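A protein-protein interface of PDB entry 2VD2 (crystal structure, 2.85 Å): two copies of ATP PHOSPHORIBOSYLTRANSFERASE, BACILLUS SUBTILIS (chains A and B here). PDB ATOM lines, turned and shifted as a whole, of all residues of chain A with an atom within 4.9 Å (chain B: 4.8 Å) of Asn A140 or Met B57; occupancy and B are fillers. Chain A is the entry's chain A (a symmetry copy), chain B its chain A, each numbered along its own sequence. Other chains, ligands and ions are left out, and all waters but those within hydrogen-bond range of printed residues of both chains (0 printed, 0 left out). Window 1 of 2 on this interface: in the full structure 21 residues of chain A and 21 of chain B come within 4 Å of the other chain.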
ATOM      1  N   LYS A 118     -23.976 -15.803  -2.812  1.00  0.00           N
ATOM      2  CA  LYS A 118     -23.248 -14.725  -3.423  1.00  0.00           C
ATOM      3  C   LYS A 118     -24.094 -13.467  -3.319  1.00  0.00           C
ATOM      4  O   LYS A 118     -23.580 -12.386  -3.493  1.00  0.00           O
ATOM      5  CB  LYS A 118     -22.972 -15.007  -4.881  1.00  0.00           C
ATOM      6  CG  LYS A 118     -22.371 -16.331  -5.194  1.00  0.00           C
ATOM      7  CD  LYS A 118     -22.037 -16.357  -6.680  1.00  0.00           C
ATOM      8  CE  LYS A 118     -21.464 -17.694  -7.173  1.00  0.00           C
ATOM      9  NZ  LYS A 118     -20.737 -17.526  -8.504  1.00  0.00           N
ATOM     10  N   LYS A 138     -22.272 -13.661   2.887  1.00  0.00           N
ATOM     11  CA  LYS A 138     -21.911 -13.388   1.505  1.00  0.00           C
ATOM     12  C   LYS A 138     -20.785 -14.322   1.230  1.00  0.00           C
ATOM     13  O   LYS A 138     -19.881 -14.454   2.046  1.00  0.00           O
ATOM     14  CB  LYS A 138     -21.517 -11.923   1.251  1.00  0.00           C
ATOM     15  CG  LYS A 138     -20.356 -11.407   2.058  1.00  0.00           C
ATOM     16  N   LEU A 139     -20.877 -15.024   0.116  1.00  0.00           N
ATOM     17  CA  LEU A 139     -19.873 -16.008  -0.258  1.00  0.00           C
ATOM     18  C   LEU A 139     -19.551 -15.678  -1.713  1.00  0.00           C
ATOM     19  O   LEU A 139     -20.449 -15.294  -2.475  1.00  0.00           O
ATOM     20  CB  LEU A 139     -20.437 -17.421  -0.071  1.00  0.00           C
ATOM     21  CG  LEU A 139     -19.567 -18.567   0.459  1.00  0.00           C
ATOM     22  CD1 LEU A 139     -18.652 -18.161   1.609  1.00  0.00           C
ATOM     23  CD2 LEU A 139     -20.468 -19.716   0.900  1.00  0.00           C
ATOM     24  N   ASN A 140     -18.278 -15.761  -2.084  1.00  0.00           N
ATOM     25  CA  ASN A 140     -17.856 -15.342  -3.410  1.00  0.00           C
ATOM     26  C   ASN A 140     -17.781 -16.474  -4.423  1.00  0.00           C
ATOM     27  O   ASN A 140     -17.457 -16.244  -5.580  1.00  0.00           O
ATOM     28  CB  ASN A 140     -16.524 -14.591  -3.335  1.00  0.00           C
ATOM     29  CG  ASN A 140     -16.705 -13.139  -2.936  1.00  0.00           C
ATOM     30  OD1 ASN A 140     -16.761 -12.811  -1.749  1.00  0.00           O
ATOM     31  ND2 ASN A 140     -16.813 -12.257  -3.932  1.00  0.00           N
ATOM     32  N   GLY A 141     -18.092 -17.690  -4.004  1.00  0.00           N
ATOM     33  CA  GLY A 141     -18.079 -18.828  -4.916  1.00  0.00           C
ATOM     34  C   GLY A 141     -18.175 -20.139  -4.169  1.00  0.00           C
ATOM     35  O   GLY A 141     -18.277 -20.154  -2.946  1.00  0.00           O
ATOM     36  N   SER A 142     -18.167 -21.246  -4.902  1.00  0.00           N
ATOM     37  CA  SER A 142     -18.153 -22.557  -4.278  1.00  0.00           C
ATOM     38  C   SER A 142     -19.253 -22.630  -3.221  1.00  0.00           C
ATOM     39  O   SER A 142     -18.994 -22.957  -2.059  1.00  0.00           O
ATOM     40  CB  SER A 142     -16.776 -22.804  -3.636  1.00  0.00           C
ATOM     41  OG  SER A 142     -15.701 -22.363  -4.465  1.00  0.00           O
ATOM     42  N   LYS B  55     -12.914 -20.239  -2.474  1.00  0.00           N
ATOM     43  CA  LYS B  55     -12.574 -19.076  -3.277  1.00  0.00           C
ATOM     44  C   LYS B  55     -11.901 -18.145  -2.266  1.00  0.00           C
ATOM     45  O   LYS B  55     -12.351 -18.039  -1.115  1.00  0.00           O
ATOM     46  CB  LYS B  55     -13.826 -18.425  -3.847  1.00  0.00           C
ATOM     47  CG  LYS B  55     -13.682 -17.910  -5.252  1.00  0.00           C
ATOM     48  CD  LYS B  55     -14.199 -18.894  -6.305  1.00  0.00           C
ATOM     49  CE  LYS B  55     -14.038 -18.306  -7.700  1.00  0.00           C
ATOM     50  NZ  LYS B  55     -15.012 -18.857  -8.672  1.00  0.00           N
ATOM     51  N   PRO B  56     -10.809 -17.491  -2.666  1.00  0.00           N
ATOM     52  CA  PRO B  56      -9.949 -16.771  -1.709  1.00  0.00           C
ATOM     53  C   PRO B  56     -10.604 -15.657  -0.884  1.00  0.00           C
ATOM     54  O   PRO B  56     -10.161 -15.408   0.224  1.00  0.00           O
ATOM     55  CB  PRO B  56      -8.832 -16.206  -2.586  1.00  0.00           C
ATOM     56  CG  PRO B  56      -9.379 -16.253  -3.975  1.00  0.00           C
ATOM     57  CD  PRO B  56     -10.306 -17.398  -4.044  1.00  0.00           C
ATOM     58  N   MET B  57     -11.636 -14.989  -1.386  1.00  0.00           N
ATOM     59  CA  MET B  57     -12.307 -14.004  -0.539  1.00  0.00           C
ATOM     60  C   MET B  57     -13.037 -14.683   0.622  1.00  0.00           C
ATOM     61  O   MET B  57     -13.258 -14.076   1.669  1.00  0.00           O
ATOM     62  CB  MET B  57     -13.267 -13.144  -1.339  1.00  0.00           C
ATOM     63  CG  MET B  57     -12.559 -12.178  -2.261  1.00  0.00           C
ATOM     64  SD  MET B  57     -11.695 -10.877  -1.365  1.00  0.00           S
ATOM     65  CE  MET B  57     -12.952  -9.580  -1.360  1.00  0.00           C
ATOM     66  N   ASP B  58     -13.390 -15.950   0.445  1.00  0.00           N
ATOM     67  CA  ASP B  58     -14.173 -16.670   1.436  1.00  0.00           C
ATOM     68  C   ASP B  58     -13.328 -17.315   2.526  1.00  0.00           C
ATOM     69  O   ASP B  58     -13.829 -17.694   3.583  1.00  0.00           O
ATOM     70  CB  ASP B  58     -14.955 -17.770   0.744  1.00  0.00           C
ATOM     71  CG  ASP B  58     -15.852 -17.249  -0.325  1.00  0.00           C
ATOM     72  OD1 ASP B  58     -16.482 -16.188  -0.092  1.00  0.00           O
ATOM     73  OD2 ASP B  58     -15.927 -17.911  -1.388  1.00  0.00           O
ATOM     74  N   VAL B  59     -12.045 -17.474   2.263  1.00  0.00           N
ATOM     75  CA  VAL B  59     -11.268 -18.273   3.153  1.00  0.00           C
ATOM     76  C   VAL B  59     -11.570 -17.796   4.545  1.00  0.00           C
ATOM     77  O   VAL B  59     -11.967 -18.593   5.398  1.00  0.00           O
ATOM     78  CB  VAL B  59      -9.777 -18.245   2.855  1.00  0.00           C
ATOM     79  CG1 VAL B  59      -9.011 -18.931   3.975  1.00  0.00           C
ATOM     80  CG2 VAL B  59      -9.523 -18.989   1.576  1.00  0.00           C
ATOM     81  N   THR B  60     -11.443 -16.504   4.791  1.00  0.00           N
ATOM     82  CA  THR B  60     -11.726 -16.052   6.134  1.00  0.00           C
ATOM     83  C   THR B  60     -13.151 -16.459   6.492  1.00  0.00           C
ATOM     84  O   THR B  60     -13.361 -17.186   7.465  1.00  0.00           O
ATOM     85  CB  THR B  60     -11.503 -14.579   6.312  1.00  0.00           C
ATOM     86  OG1 THR B  60     -10.132 -14.281   6.022  1.00  0.00           O
ATOM     87  CG2 THR B  60     -11.834 -14.154   7.739  1.00  0.00           C
ATOM     88  N   THR B  61     -14.134 -16.058   5.691  1.00  0.00           N
ATOM     89  CA  THR B  61     -15.508 -16.486   5.981  1.00  0.00           C
ATOM     90  C   THR B  61     -15.494 -17.834   6.713  1.00  0.00           C
ATOM     91  O   THR B  61     -15.789 -17.922   7.912  1.00  0.00           O
ATOM     92  CB  THR B  61     -16.334 -16.647   4.722  1.00  0.00           C
ATOM     93  OG1 THR B  61     -16.080 -15.545   3.850  1.00  0.00           O
ATOM     94  CG2 THR B  61     -17.784 -16.716   5.071  1.00  0.00           C
ATOM     95  N   ASP B  76      -6.224 -10.907   0.168  1.00  0.00           N
ATOM     96  CA  ASP B  76      -7.445 -10.660  -0.600  1.00  0.00           C
ATOM     97  C   ASP B  76      -8.660 -10.703   0.333  1.00  0.00           C
ATOM     98  O   ASP B  76      -9.473  -9.783   0.323  1.00  0.00           O
ATOM     99  CB  ASP B  76      -7.627 -11.708  -1.717  1.00  0.00           C
ATOM    100  CG  ASP B  76      -6.338 -11.984  -2.511  1.00  0.00           C
ATOM    101  OD1 ASP B  76      -5.340 -12.438  -1.901  1.00  0.00           O
ATOM    102  OD2 ASP B  76      -6.332 -11.792  -3.752  1.00  0.00           O
ATOM    103  N   VAL B  77      -8.773 -11.756   1.150  1.00  0.00           N
ATOM    104  CA  VAL B  77      -9.853 -11.843   2.155  1.00  0.00           C
ATOM    105  C   VAL B  77      -9.868 -10.600   3.051  1.00  0.00           C
ATOM    106  O   VAL B  77     -10.898  -9.931   3.225  1.00  0.00           O
ATOM    107  CB  VAL B  77      -9.749 -13.086   3.111  1.00  0.00           C
ATOM    108  CG1 VAL B  77     -11.143 -13.612   3.437  1.00  0.00           C
ATOM    109  CG2 VAL B  77      -8.893 -14.196   2.521  1.00  0.00           C
ATOM    110  N   GLU B  80     -11.394  -7.236   2.214  1.00  0.00           N
ATOM    111  CA  GLU B  80     -12.803  -6.987   2.572  1.00  0.00           C
ATOM    112  C   GLU B  80     -12.968  -5.798   3.559  1.00  0.00           C
ATOM    113  O   GLU B  80     -13.444  -4.729   3.157  1.00  0.00           O
ATOM    114  CB  GLU B  80     -13.442  -8.266   3.132  1.00  0.00           C
ATOM    115  N   ARG B  83     -12.327  -7.610  10.698  1.00  0.00           N
ATOM    116  CA  ARG B  83     -13.158  -8.782  11.035  1.00  0.00           C
ATOM    117  C   ARG B  83     -12.464  -9.766  12.005  1.00  0.00           C
ATOM    118  O   ARG B  83     -11.265  -9.641  12.267  1.00  0.00           O
ATOM    119  CB  ARG B  83     -13.517  -9.532   9.754  1.00  0.00           C
ATOM    120  CG  ARG B  83     -12.340 -10.305   9.140  1.00  0.00           C
ATOM    121  CD  ARG B  83     -12.619 -10.714   7.703  1.00  0.00           C
ATOM    122  NE  ARG B  83     -13.979 -11.238   7.525  1.00  0.00           N
ATOM    123  CZ  ARG B  83     -14.370 -12.027   6.520  1.00  0.00           C
ATOM    124  NH1 ARG B  83     -15.641 -12.431   6.452  1.00  0.00           N
ATOM    125  NH2 ARG B  83     -13.512 -12.412   5.575  1.00  0.00           N
ATOM    126  N   TYR B 119     -12.878  -4.377  -5.947  1.00  0.00           N
ATOM    127  CA  TYR B 119     -12.812  -3.956  -4.564  1.00  0.00           C
ATOM    128  C   TYR B 119     -13.162  -2.505  -4.356  1.00  0.00           C
ATOM    129  O   TYR B 119     -12.283  -1.708  -4.024  1.00  0.00           O
ATOM    130  CB  TYR B 119     -11.409  -4.202  -4.049  1.00  0.00           C
ATOM    131  CG  TYR B 119     -10.905  -5.504  -4.542  1.00  0.00           C
ATOM    132  CD1 TYR B 119     -11.601  -6.681  -4.273  1.00  0.00           C
ATOM    133  CD2 TYR B 119      -9.773  -5.567  -5.332  1.00  0.00           C
ATOM    134  CE1 TYR B 119     -11.156  -7.900  -4.749  1.00  0.00           C
ATOM    135  CE2 TYR B 119      -9.309  -6.778  -5.816  1.00  0.00           C
ATOM    136  CZ  TYR B 119     -10.000  -7.944  -5.519  1.00  0.00           C
ATOM    137  OH  TYR B 119      -9.532  -9.146  -6.015  1.00  0.00           O
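Of the 12 printed residues of chain B, 3 touch a printed residue of chain A. Hydrophobic or aromatic side chains of chain B within 4 Å of the printed part of chain A: Met B57. Along chain B the printed residues that touch a printed residue of chain A span positions 57 to 61. Of the 6 printed residues of chain A, 3 touch a printed residue of chain B. Hydrophobic or aromatic side chains of chain A within 4 Å of the printed part of chain B: Leu A139. Along chain A the printed residues that touch a printed residue of chain B span positions 139 to 141. Among the printed residues, no Asp or Glu carboxylate lies within 4 Å of a Lys or Arg side-chain nitrogen of the other chain.
No position is printed for both chains. Of the 5 pairs that touch across the chains among the printed residues, none has its exchanged pair printed and touching as well.
The side-chain carboxylate (OD1) of Asp B58 is in hydrogen-bond range of the backbone NH (N) of Asn A140, at 2.7 Å. The side-chain carboxylate (OD2) of Asp B58 lies within hydrogen-bond range of the backbone NH (N) of Gly A141, at 3.4 Å.
Among the printed residues, pairs that only touch across the chains: Leu A139 with Asp B58, Leu A139 with Thr B61 and Asn A140 with Met B57.
The backbone carbonyl oxygen of Asp B58 sits close to the side-chain hydroxyl of Thr B61 (3.1 Å).
Asn A140 touches just these residues of chain B: Met B57 (3.5 Å) and Asp B58 (2.7 Å). Met B57 touches just one residue of chain A: Asn A140 (3.5 Å). Of the printed residues of chain B, Leu A139 touches Asp B58 and Thr B61. Of the printed residues of chain A, Asp B58 touches Leu A139 (3.4 Å), Asn A140 (2.7 Å) and Gly A141 (3.4 Å). Of the printed residues of chain A, Thr B61 touches Leu A139 (3.9 Å). Printed residues of chain B within 4 Å of Gly A141: Asp B58. The nearest printed residue of chain A that does not touch Met B57 is Lys A138 (6.6 Å). The nearest printed residue of chain A that does not touch Asp B58 is Lys A138 (4.4 Å).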
